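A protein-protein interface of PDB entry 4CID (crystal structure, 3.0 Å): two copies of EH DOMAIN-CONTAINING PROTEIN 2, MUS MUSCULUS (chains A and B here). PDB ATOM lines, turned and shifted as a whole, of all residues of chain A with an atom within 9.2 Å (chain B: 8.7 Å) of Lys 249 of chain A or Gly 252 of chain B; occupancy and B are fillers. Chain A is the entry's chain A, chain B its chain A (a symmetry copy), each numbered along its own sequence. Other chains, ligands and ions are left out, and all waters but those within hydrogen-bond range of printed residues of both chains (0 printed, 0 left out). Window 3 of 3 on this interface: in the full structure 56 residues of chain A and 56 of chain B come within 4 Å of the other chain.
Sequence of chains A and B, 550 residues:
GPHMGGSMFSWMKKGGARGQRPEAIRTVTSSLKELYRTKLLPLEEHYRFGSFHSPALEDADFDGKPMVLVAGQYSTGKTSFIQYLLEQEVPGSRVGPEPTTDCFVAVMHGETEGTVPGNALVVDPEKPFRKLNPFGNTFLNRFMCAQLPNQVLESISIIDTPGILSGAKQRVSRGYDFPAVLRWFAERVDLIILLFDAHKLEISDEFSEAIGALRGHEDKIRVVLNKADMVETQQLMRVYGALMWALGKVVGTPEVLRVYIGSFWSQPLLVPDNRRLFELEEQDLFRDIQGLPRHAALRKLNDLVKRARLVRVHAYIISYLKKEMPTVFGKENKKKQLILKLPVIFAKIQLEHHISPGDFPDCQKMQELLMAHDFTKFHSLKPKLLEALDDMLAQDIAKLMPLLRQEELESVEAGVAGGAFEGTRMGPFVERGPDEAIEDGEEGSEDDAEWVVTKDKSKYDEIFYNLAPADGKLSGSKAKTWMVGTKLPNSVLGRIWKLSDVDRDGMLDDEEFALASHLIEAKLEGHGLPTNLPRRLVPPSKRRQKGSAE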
ATOM      1  N   ILE A 203     -13.720 -20.055  -7.694  1.00  0.00           N
ATOM      2  CA  ILE A 203     -13.318 -21.457  -7.545  1.00  0.00           C
ATOM      3  C   ILE A 203     -13.838 -21.932  -6.175  1.00  0.00           C
ATOM      4  O   ILE A 203     -13.141 -21.859  -5.161  1.00  0.00           O
ATOM      5  CB  ILE A 203     -11.783 -21.653  -7.757  1.00  0.00           C
ATOM      6  CG1 ILE A 203     -11.359 -23.105  -7.489  1.00  0.00           C
ATOM      7  CG2 ILE A 203     -10.952 -20.681  -6.919  1.00  0.00           C
ATOM      8  CD1 ILE A 203     -11.976 -24.112  -8.429  1.00  0.00           C
ATOM      9  N   SER A 208     -14.334 -27.614  -5.739  1.00  0.00           N
ATOM     10  CA  SER A 208     -13.117 -28.259  -5.214  1.00  0.00           C
ATOM     11  C   SER A 208     -13.351 -29.716  -4.815  1.00  0.00           C
ATOM     12  O   SER A 208     -12.442 -30.542  -4.886  1.00  0.00           O
ATOM     13  CB  SER A 208     -12.581 -27.489  -4.004  1.00  0.00           C
ATOM     14  OG  SER A 208     -12.302 -26.142  -4.342  1.00  0.00           O
ATOM     15  N   ILE A 211     -13.705 -31.805  -8.312  1.00  0.00           N
ATOM     16  CA  ILE A 211     -12.395 -32.184  -8.876  1.00  0.00           C
ATOM     17  C   ILE A 211     -11.846 -33.469  -8.239  1.00  0.00           C
ATOM     18  O   ILE A 211     -11.361 -34.361  -8.946  1.00  0.00           O
ATOM     19  CB  ILE A 211     -11.357 -31.045  -8.758  1.00  0.00           C
ATOM     20  CG1 ILE A 211     -11.489 -30.074  -9.935  1.00  0.00           C
ATOM     21  CG2 ILE A 211      -9.937 -31.597  -8.725  1.00  0.00           C
ATOM     22  CD1 ILE A 211     -12.718 -29.196  -9.881  1.00  0.00           C
ATOM     23  N   ARG A 215     -10.286 -37.242  -9.856  1.00  0.00           N
ATOM     24  CA  ARG A 215      -8.956 -37.786  -9.555  1.00  0.00           C
ATOM     25  C   ARG A 215      -8.740 -39.138 -10.239  1.00  0.00           C
ATOM     26  O   ARG A 215      -9.600 -40.016 -10.183  1.00  0.00           O
ATOM     27  CB  ARG A 215      -8.758 -37.914  -8.036  1.00  0.00           C
ATOM     28  CG  ARG A 215      -7.364 -38.361  -7.606  1.00  0.00           C
ATOM     29  CD  ARG A 215      -6.956 -37.761  -6.266  1.00  0.00           C
ATOM     30  NE  ARG A 215      -6.809 -36.302  -6.336  1.00  0.00           N
ATOM     31  CZ  ARG A 215      -6.427 -35.519  -5.325  1.00  0.00           C
ATOM     32  NH1 ARG A 215      -6.138 -36.036  -4.135  1.00  0.00           N
ATOM     33  NH2 ARG A 215      -6.329 -34.206  -5.506  1.00  0.00           N
ATOM     34  N   ALA A 242      -4.883 -16.370 -11.155  1.00  0.00           N
ATOM     35  CA  ALA A 242      -5.597 -16.853  -9.974  1.00  0.00           C
ATOM     36  C   ALA A 242      -6.142 -18.259 -10.191  1.00  0.00           C
ATOM     37  O   ALA A 242      -5.946 -19.145  -9.349  1.00  0.00           O
ATOM     38  CB  ALA A 242      -6.723 -15.901  -9.614  1.00  0.00           C
ATOM     39  N   LEU A 243      -6.803 -18.468 -11.328  1.00  0.00           N
ATOM     40  CA  LEU A 243      -7.344 -19.792 -11.643  1.00  0.00           C
ATOM     41  C   LEU A 243      -6.288 -20.908 -11.570  1.00  0.00           C
ATOM     42  O   LEU A 243      -6.545 -21.971 -11.001  1.00  0.00           O
ATOM     43  CB  LEU A 243      -7.990 -19.788 -13.027  1.00  0.00           C
ATOM     44  CG  LEU A 243      -8.575 -21.110 -13.522  1.00  0.00           C
ATOM     45  CD1 LEU A 243      -9.663 -21.618 -12.590  1.00  0.00           C
ATOM     46  CD2 LEU A 243      -9.123 -20.929 -14.923  1.00  0.00           C
ATOM     47  N   MET A 244      -5.107 -20.664 -12.136  1.00  0.00           N
ATOM     48  CA  MET A 244      -4.061 -21.691 -12.174  1.00  0.00           C
ATOM     49  C   MET A 244      -3.449 -21.847 -10.822  1.00  0.00           C
ATOM     50  O   MET A 244      -3.155 -22.968 -10.398  1.00  0.00           O
ATOM     51  CB  MET A 244      -2.941 -21.357 -13.153  1.00  0.00           C
ATOM     52  CG  MET A 244      -3.429 -21.391 -14.603  1.00  0.00           C
ATOM     53  SD  MET A 244      -3.859 -23.229 -15.186  1.00  0.00           S
ATOM     54  CE  MET A 244      -2.139 -23.642 -16.041  1.00  0.00           C
ATOM     55  N   TRP A 245      -3.238 -20.723 -10.139  1.00  0.00           N
ATOM     56  CA  TRP A 245      -2.777 -20.747  -8.750  1.00  0.00           C
ATOM     57  C   TRP A 245      -3.686 -21.624  -7.905  1.00  0.00           C
ATOM     58  O   TRP A 245      -3.210 -22.413  -7.087  1.00  0.00           O
ATOM     59  CB  TRP A 245      -2.776 -19.336  -8.178  1.00  0.00           C
ATOM     60  CG  TRP A 245      -2.217 -19.212  -6.798  1.00  0.00           C
ATOM     61  CD1 TRP A 245      -2.835 -19.533  -5.624  1.00  0.00           C
ATOM     62  CD2 TRP A 245      -0.938 -18.690  -6.447  1.00  0.00           C
ATOM     63  NE1 TRP A 245      -2.010 -19.256  -4.563  1.00  0.00           N
ATOM     64  CE2 TRP A 245      -0.837 -18.735  -5.042  1.00  0.00           C
ATOM     65  CE3 TRP A 245       0.139 -18.193  -7.186  1.00  0.00           C
ATOM     66  CZ2 TRP A 245       0.301 -18.303  -4.363  1.00  0.00           C
ATOM     67  CZ3 TRP A 245       1.269 -17.767  -6.511  1.00  0.00           C
ATOM     68  CH2 TRP A 245       1.342 -17.822  -5.117  1.00  0.00           C
ATOM     69  N   ALA A 246      -4.994 -21.470  -8.108  1.00  0.00           N
ATOM     70  CA  ALA A 246      -5.984 -22.284  -7.409  1.00  0.00           C
ATOM     71  C   ALA A 246      -5.917 -23.753  -7.833  1.00  0.00           C
ATOM     72  O   ALA A 246      -5.617 -24.630  -7.014  1.00  0.00           O
ATOM     73  CB  ALA A 246      -7.377 -21.731  -7.651  1.00  0.00           C
ATOM     74  N   LEU A 247      -6.177 -24.009  -9.114  1.00  0.00           N
ATOM     75  CA  LEU A 247      -6.201 -25.371  -9.646  1.00  0.00           C
ATOM     76  C   LEU A 247      -4.933 -26.155  -9.330  1.00  0.00           C
ATOM     77  O   LEU A 247      -4.988 -27.371  -9.135  1.00  0.00           O
ATOM     78  CB  LEU A 247      -6.419 -25.358 -11.158  1.00  0.00           C
ATOM     79  CG  LEU A 247      -7.848 -25.130 -11.641  1.00  0.00           C
ATOM     80  CD1 LEU A 247      -7.850 -25.020 -13.155  1.00  0.00           C
ATOM     81  CD2 LEU A 247      -8.779 -26.243 -11.186  1.00  0.00           C
ATOM     82  N   GLY A 248      -3.799 -25.459  -9.290  1.00  0.00           N
ATOM     83  CA  GLY A 248      -2.546 -26.055  -8.842  1.00  0.00           C
ATOM     84  C   GLY A 248      -2.705 -26.799  -7.529  1.00  0.00           C
ATOM     85  O   GLY A 248      -2.315 -27.966  -7.427  1.00  0.00           O
ATOM     86  N   LYS A 249      -3.303 -26.138  -6.538  1.00  0.00           N
ATOM     87  CA  LYS A 249      -3.465 -26.727  -5.206  1.00  0.00           C
ATOM     88  C   LYS A 249      -4.528 -27.813  -5.168  1.00  0.00           C
ATOM     89  O   LYS A 249      -4.390 -28.795  -4.444  1.00  0.00           O
ATOM     90  CB  LYS A 249      -3.812 -25.653  -4.181  1.00  0.00           C
ATOM     91  CG  LYS A 249      -2.718 -24.613  -4.006  1.00  0.00           C
ATOM     92  CD  LYS A 249      -3.052 -23.595  -2.924  1.00  0.00           C
ATOM     93  CE  LYS A 249      -2.906 -24.178  -1.523  1.00  0.00           C
ATOM     94  NZ  LYS A 249      -3.083 -23.139  -0.468  1.00  0.00           N
ATOM     95  N   VAL A 250      -5.577 -27.643  -5.961  1.00  0.00           N
ATOM     96  CA  VAL A 250      -6.743 -28.512  -5.877  1.00  0.00           C
ATOM     97  C   VAL A 250      -6.487 -29.901  -6.464  1.00  0.00           C
ATOM     98  O   VAL A 250      -6.678 -30.898  -5.767  1.00  0.00           O
ATOM     99  CB  VAL A 250      -7.976 -27.868  -6.542  1.00  0.00           C
ATOM    100  CG1 VAL A 250      -9.188 -28.786  -6.445  1.00  0.00           C
ATOM    101  CG2 VAL A 250      -8.291 -26.527  -5.885  1.00  0.00           C
ATOM    102  N   VAL A 251      -6.067 -29.981  -7.728  1.00  0.00           N
ATOM    103  CA  VAL A 251      -5.797 -31.294  -8.342  1.00  0.00           C
ATOM    104  C   VAL A 251      -4.488 -31.877  -7.812  1.00  0.00           C
ATOM    105  O   VAL A 251      -4.344 -33.097  -7.720  1.00  0.00           O
ATOM    106  CB  VAL A 251      -5.755 -31.272  -9.890  1.00  0.00           C
ATOM    107  CG1 VAL A 251      -7.033 -30.689 -10.477  1.00  0.00           C
ATOM    108  CG2 VAL A 251      -4.557 -30.505 -10.404  1.00  0.00           C
ATOM    109  N   GLY A 252      -3.529 -31.005  -7.495  1.00  0.00           N
ATOM    110  CA  GLY A 252      -2.294 -31.412  -6.824  1.00  0.00           C
ATOM    111  C   GLY A 252      -1.257 -32.150  -7.661  1.00  0.00           C
ATOM    112  O   GLY A 252      -0.114 -32.302  -7.226  1.00  0.00           O
ATOM    113  N   THR A 253      -1.641 -32.619  -8.848  1.00  0.00           N
ATOM    114  CA  THR A 253      -0.718 -33.319  -9.744  1.00  0.00           C
ATOM    115  C   THR A 253       0.431 -32.403 -10.200  1.00  0.00           C
ATOM    116  O   THR A 253       0.237 -31.196 -10.342  1.00  0.00           O
ATOM    117  CB  THR A 253      -1.458 -33.895 -10.979  1.00  0.00           C
ATOM    118  OG1 THR A 253      -0.572 -34.737 -11.728  1.00  0.00           O
ATOM    119  CG2 THR A 253      -1.998 -32.786 -11.895  1.00  0.00           C
ATOM    120  N   ILE B 211      12.294 -19.711  -1.886  1.00  0.00           N
ATOM    121  CA  ILE B 211      10.965 -19.189  -1.515  1.00  0.00           C
ATOM    122  C   ILE B 211      10.626 -19.475  -0.044  1.00  0.00           C
ATOM    123  O   ILE B 211      10.142 -18.589   0.671  1.00  0.00           O
ATOM    124  CB  ILE B 211       9.847 -19.730  -2.434  1.00  0.00           C
ATOM    125  CG1 ILE B 211       9.735 -18.877  -3.702  1.00  0.00           C
ATOM    126  CG2 ILE B 211       8.502 -19.736  -1.719  1.00  0.00           C
ATOM    127  CD1 ILE B 211      10.871 -19.067  -4.680  1.00  0.00           C
ATOM    128  N   ARG B 215       9.239 -16.990   3.300  1.00  0.00           N
ATOM    129  CA  ARG B 215       8.015 -17.245   4.071  1.00  0.00           C
ATOM    130  C   ARG B 215       7.843 -16.223   5.197  1.00  0.00           C
ATOM    131  O   ARG B 215       8.783 -15.940   5.939  1.00  0.00           O
ATOM    132  CB  ARG B 215       8.025 -18.674   4.639  1.00  0.00           C
ATOM    133  CG  ARG B 215       6.746 -19.086   5.361  1.00  0.00           C
ATOM    134  CD  ARG B 215       6.457 -20.576   5.213  1.00  0.00           C
ATOM    135  NE  ARG B 215       6.164 -20.945   3.823  1.00  0.00           N
ATOM    136  CZ  ARG B 215       5.842 -22.171   3.406  1.00  0.00           C
ATOM    137  NH1 ARG B 215       5.757 -23.182   4.265  1.00  0.00           N
ATOM    138  NH2 ARG B 215       5.598 -22.388   2.118  1.00  0.00           N
ATOM    139  N   GLU B 218       5.570 -12.508   2.230  1.00  0.00           N
ATOM    140  CA  GLU B 218       4.952 -12.717   0.921  1.00  0.00           C
ATOM    141  C   GLU B 218       4.652 -11.352   0.300  1.00  0.00           C
ATOM    142  O   GLU B 218       4.924 -11.112  -0.877  1.00  0.00           O
ATOM    143  CB  GLU B 218       3.639 -13.524   1.023  1.00  0.00           C
ATOM    144  CG  GLU B 218       3.503 -14.547   2.162  1.00  0.00           C
ATOM    145  CD  GLU B 218       4.480 -15.709   2.083  1.00  0.00           C
ATOM    146  OE1 GLU B 218       5.153 -15.864   1.043  1.00  0.00           O
ATOM    147  OE2 GLU B 218       4.563 -16.479   3.067  1.00  0.00           O
ATOM    148  N   MET B 244       2.260 -20.113 -12.460  1.00  0.00           N
ATOM    149  CA  MET B 244       1.320 -19.879 -11.360  1.00  0.00           C
ATOM    150  C   MET B 244       0.903 -21.180 -10.759  1.00  0.00           C
ATOM    151  O   MET B 244       0.773 -21.287  -9.536  1.00  0.00           O
ATOM    152  CB  MET B 244       0.058 -19.150 -11.806  1.00  0.00           C
ATOM    153  CG  MET B 244       0.358 -17.713 -12.238  1.00  0.00           C
ATOM    154  SD  MET B 244       0.882 -16.585 -10.704  1.00  0.00           S
ATOM    155  CE  MET B 244      -0.885 -15.814 -10.328  1.00  0.00           C
ATOM    156  N   TRP B 245       0.674 -22.176 -11.613  1.00  0.00           N
ATOM    157  CA  TRP B 245       0.399 -23.536 -11.147  1.00  0.00           C
ATOM    158  C   TRP B 245       1.487 -24.000 -10.193  1.00  0.00           C
ATOM    159  O   TRP B 245       1.196 -24.595  -9.154  1.00  0.00           O
ATOM    160  CB  TRP B 245       0.336 -24.489 -12.332  1.00  0.00           C
ATOM    161  CG  TRP B 245      -0.052 -25.893 -11.996  1.00  0.00           C
ATOM    162  CD1 TRP B 245       0.738 -26.859 -11.444  1.00  0.00           C
ATOM    163  CD2 TRP B 245      -1.319 -26.500 -12.234  1.00  0.00           C
ATOM    164  NE1 TRP B 245       0.033 -28.028 -11.309  1.00  0.00           N
ATOM    165  CE2 TRP B 245      -1.235 -27.834 -11.789  1.00  0.00           C
ATOM    166  CE3 TRP B 245      -2.524 -26.042 -12.774  1.00  0.00           C
ATOM    167  CZ2 TRP B 245      -2.314 -28.714 -11.867  1.00  0.00           C
ATOM    168  CZ3 TRP B 245      -3.594 -26.916 -12.849  1.00  0.00           C
ATOM    169  CH2 TRP B 245      -3.483 -28.235 -12.402  1.00  0.00           C
ATOM    170  N   ALA B 246       2.738 -23.727 -10.563  1.00  0.00           N
ATOM    171  CA  ALA B 246       3.882 -24.063  -9.720  1.00  0.00           C
ATOM    172  C   ALA B 246       3.901 -23.240  -8.430  1.00  0.00           C
ATOM    173  O   ALA B 246       3.792 -23.794  -7.329  1.00  0.00           O
ATOM    174  CB  ALA B 246       5.173 -23.861 -10.491  1.00  0.00           C
ATOM    175  N   LEU B 247       4.019 -21.921  -8.574  1.00  0.00           N
ATOM    176  CA  LEU B 247       4.104 -21.018  -7.427  1.00  0.00           C
ATOM    177  C   LEU B 247       2.967 -21.211  -6.432  1.00  0.00           C
ATOM    178  O   LEU B 247       3.161 -21.040  -5.227  1.00  0.00           O
ATOM    179  CB  LEU B 247       4.125 -19.561  -7.886  1.00  0.00           C
ATOM    180  CG  LEU B 247       5.453 -19.031  -8.419  1.00  0.00           C
ATOM    181  CD1 LEU B 247       5.251 -17.620  -8.944  1.00  0.00           C
ATOM    182  CD2 LEU B 247       6.536 -19.053  -7.352  1.00  0.00           C
ATOM    183  N   GLY B 248       1.786 -21.559  -6.939  1.00  0.00           N
ATOM    184  CA  GLY B 248       0.663 -21.932  -6.088  1.00  0.00           C
ATOM    185  C   GLY B 248       1.058 -22.952  -5.035  1.00  0.00           C
ATOM    186  O   GLY B 248       0.796 -22.748  -3.846  1.00  0.00           O
ATOM    187  N   LYS B 249       1.712 -24.031  -5.467  1.00  0.00           N
ATOM    188  CA  LYS B 249       2.097 -25.113  -4.557  1.00  0.00           C
ATOM    189  C   LYS B 249       3.255 -24.734  -3.647  1.00  0.00           C
ATOM    190  O   LYS B 249       3.304 -25.151  -2.494  1.00  0.00           O
ATOM    191  CB  LYS B 249       2.469 -26.368  -5.341  1.00  0.00           C
ATOM    192  CG  LYS B 249       1.312 -26.939  -6.143  1.00  0.00           C
ATOM    193  CD  LYS B 249       1.682 -28.233  -6.856  1.00  0.00           C
ATOM    194  CE  LYS B 249       1.772 -29.412  -5.893  1.00  0.00           C
ATOM    195  NZ  LYS B 249       1.983 -30.701  -6.613  1.00  0.00           N
ATOM    196  N   VAL B 250       4.173 -23.928  -4.163  1.00  0.00           N
ATOM    197  CA  VAL B 250       5.418 -23.645  -3.460  1.00  0.00           C
ATOM    198  C   VAL B 250       5.222 -22.708  -2.268  1.00  0.00           C
ATOM    199  O   VAL B 250       5.594 -23.065  -1.149  1.00  0.00           O
ATOM    200  CB  VAL B 250       6.489 -23.082  -4.415  1.00  0.00           C
ATOM    201  CG1 VAL B 250       7.785 -22.793  -3.668  1.00  0.00           C
ATOM    202  CG2 VAL B 250       6.757 -24.066  -5.551  1.00  0.00           C
ATOM    203  N   VAL B 251       4.654 -21.521  -2.488  1.00  0.00           N
ATOM    204  CA  VAL B 251       4.434 -20.581  -1.374  1.00  0.00           C
ATOM    205  C   VAL B 251       3.265 -21.042  -0.504  1.00  0.00           C
ATOM    206  O   VAL B 251       3.250 -20.790   0.701  1.00  0.00           O
ATOM    207  CB  VAL B 251       4.194 -19.118  -1.818  1.00  0.00           C
ATOM    208  CG1 VAL B 251       5.324 -18.606  -2.698  1.00  0.00           C
ATOM    209  CG2 VAL B 251       2.872 -18.965  -2.538  1.00  0.00           C
ATOM    210  N   GLY B 252       2.275 -21.688  -1.125  1.00  0.00           N
ATOM    211  CA  GLY B 252       1.180 -22.326  -0.394  1.00  0.00           C
ATOM    212  C   GLY B 252       0.120 -21.414   0.209  1.00  0.00           C
ATOM    213  O   GLY B 252      -0.939 -21.893   0.619  1.00  0.00           O
ATOM    214  N   THR B 253       0.392 -20.110   0.278  1.00  0.00           N
ATOM    215  CA  THR B 253      -0.567 -19.142   0.814  1.00  0.00           C
ATOM    216  C   THR B 253      -1.846 -19.082  -0.039  1.00  0.00           C
ATOM    217  O   THR B 253      -1.787 -19.278  -1.252  1.00  0.00           O
ATOM    218  CB  THR B 253       0.061 -17.729   0.927  1.00  0.00           C
ATOM    219  OG1 THR B 253      -0.829 -16.856   1.633  1.00  0.00           O
ATOM    220  CG2 THR B 253       0.372 -17.126  -0.453  1.00  0.00           C
ATOM    221  N   PRO B 254      -3.008 -18.822   0.593  1.00  0.00           N
ATOM    222  CA  PRO B 254      -4.239 -18.652  -0.192  1.00  0.00           C
ATOM    223  C   PRO B 254      -4.291 -17.346  -0.995  1.00  0.00           C
ATOM    224  O   PRO B 254      -5.097 -17.236  -1.920  1.00  0.00           O
ATOM    225  CB  PRO B 254      -5.348 -18.662   0.871  1.00  0.00           C
ATOM    226  CG  PRO B 254      -4.718 -19.185   2.116  1.00  0.00           C
ATOM    227  CD  PRO B 254      -3.279 -18.789   2.040  1.00  0.00           C
ATOM    228  N   GLU B 255      -3.451 -16.372  -0.639  1.00  0.00           N
ATOM    229  CA  GLU B 255      -3.406 -15.082  -1.326  1.00  0.00           C
ATOM    230  C   GLU B 255      -2.471 -15.142  -2.526  1.00  0.00           C
ATOM    231  O   GLU B 255      -1.249 -15.174  -2.370  1.00  0.00           O
ATOM    232  CB  GLU B 255      -2.933 -13.976  -0.379  1.00  0.00           C
ATOM    233  CG  GLU B 255      -3.913 -13.639   0.738  1.00  0.00           C
ATOM    234  CD  GLU B 255      -3.924 -14.660   1.862  1.00  0.00           C
ATOM    235  OE1 GLU B 255      -2.851 -15.209   2.194  1.00  0.00           O
ATOM    236  OE2 GLU B 255      -5.015 -14.919   2.413  1.00  0.00           O
ATOM    237  N   VAL B 256      -3.054 -15.151  -3.723  1.00  0.00           N
ATOM    238  CA  VAL B 256      -2.293 -15.194  -4.973  1.00  0.00           C
ATOM    239  C   VAL B 256      -1.312 -14.032  -5.103  1.00  0.00           C
ATOM    240  O   VAL B 256      -1.641 -12.898  -4.773  1.00  0.00           O
ATOM    241  CB  VAL B 256      -3.227 -15.181  -6.205  1.00  0.00           C
ATOM    242  CG1 VAL B 256      -3.973 -13.856  -6.330  1.00  0.00           C
ATOM    243  CG2 VAL B 256      -2.439 -15.455  -7.475  1.00  0.00           C
ATOM    244  N   LEU B 257      -0.114 -14.326  -5.601  1.00  0.00           N
ATOM    245  CA  LEU B 257       0.906 -13.299  -5.814  1.00  0.00           C
ATOM    246  C   LEU B 257       0.713 -12.595  -7.149  1.00  0.00           C
ATOM    247  O   LEU B 257       0.359 -13.215  -8.156  1.00  0.00           O
ATOM    248  CB  LEU B 257       2.317 -13.884  -5.738  1.00  0.00           C
ATOM    249  CG  LEU B 257       3.012 -13.730  -4.388  1.00  0.00           C
ATOM    250  CD1 LEU B 257       2.178 -14.329  -3.265  1.00  0.00           C
ATOM    251  CD2 LEU B 257       4.386 -14.377  -4.436  1.00  0.00           C
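NE1 of Trp 245 of chain A lies within hydrogen-bond range of O of Thr 253 of chain B.
NZ of Lys 249 of chain A lies within hydrogen-bond range of O of Gly 252 of chain B (2.7 Å).
The side-chain amino group (NZ) of Lys 249 of chain B lies within hydrogen-bond range of the backbone carbonyl oxygen (O) of Gly 252 of chain A (2.7 Å).
The backbone carbonyl oxygen (O) of Thr 253 of chain A lies within hydrogen-bond range of the indole nitrogen (NE1) of Trp 245 of chain B (3.3 Å).
The guanidinium group (NH2) of Arg 215 of chain A lies within hydrogen-bond range of the backbone carbonyl oxygen (O) of Val 251 of chain A.
The guanidinium group (NH2) of Arg 215 of chain B sits at hydrogen-bond distance from the backbone carbonyl oxygen (O) of Val 251 of chain B (3.2 Å).
The side-chain hydroxyl of Thr 253 of chain B lies within hydrogen-bond range of the side-chain carboxylate of Glu 255 of chain B, 2.7 Å away.
Among the printed residues, merely in contact across the chains: Met 244 of chain A with Met 244 of chain B (3.96 Å), Met 244 of chain A with Trp 245 of chain B (3.7 Å), Trp 245 of chain A with Met 244 of chain B (3.7 Å), Trp 245 of chain A with Leu 247 of chain B (3.6 Å), Trp 245 of chain A with Gly 248 of chain B (3.6 Å), Trp 245 of chain A with Val 251 of chain B (3.2 Å), Trp 245 of chain A with Val 256 of chain B (3.7 Å), Trp 245 of chain A with Leu 257 of chain B (3.8 Å), Leu 247 of chain A with Trp 245 of chain B (3.6 Å), Gly 248 of chain A with Trp 245 of chain B (3.6 Å), Gly 248 of chain A with Lys 249 of chain B (3.98 Å), Lys 249 of chain A with Gly 248 of chain B (3.98 Å) and Val 251 of chain A with Trp 245 of chain B (3.2 Å).
Of the printed residues of chain B, Lys 249 of chain A touches Gly 248 and Gly 252.
Gly 252 of chain B touches just one residue of chain A: Lys 249 (2.7 Å).
Val 251 of chain B touches one residue of chain A.
Printed residues of chain B within 4 Å of Trp 245 of chain A: Met 244, Leu 247, Gly 248, Val 251, Thr 253, Val 256 and Leu 257.
Of the printed residues of chain A, Val 256 of chain B touches Trp 245.
Of the printed residues of chain A, Leu 257 of chain B touches Trp 245 (3.8 Å).
Of the printed residues of chain A, Met 244 of chain B touches Met 244 (3.96 Å) and Trp 245 (3.7 Å).
Glu 255 of chain B touches none of the printed residues of chain A.
Glu 218 of chain B touches none of the printed residues of chain A.
The nearest residue of chain A that does not touch Gly 252 of chain B is Trp 245 of chain A (5.1 Å).
The nearest printed residue of chain B that does not touch Trp 245 of chain A is Glu 255 of chain B (4.02 Å).
Printed residues of chain A that touch a printed residue of chain B: Met 244, Trp 245, Leu 247, Gly 248, Lys 249, Val 251, Gly 252 and Thr 253.
Among the printed residues, no Asp or Glu carboxylate lies within 4 Å of a Lys or Arg side-chain nitrogen of the other chain.
Met 244 of chain B touches its own counterpart, Met 244 of chain A.
Trp 245 of chain A touches Gly 248 of chain B, and with the chains exchanged Gly 248 of chain A touches Trp 245 of chain B.
Trp 245 of chain A touches Val 251 of chain B, and with the chains exchanged Val 251 of chain A touches Trp 245 of chain B.
Trp 245 of chain A touches Thr 253 of chain B, and with the chains exchanged Thr 253 of chain A touches Trp 245 of chain B.
Positions printed for both chains: 211, 215, 244, 245, 246, 247, 248, 249, 250, 251, 252 and 253.
Of the 17 pairs that touch across the chains among the printed residues, 15 have their exchanged pair printed and touching as well.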
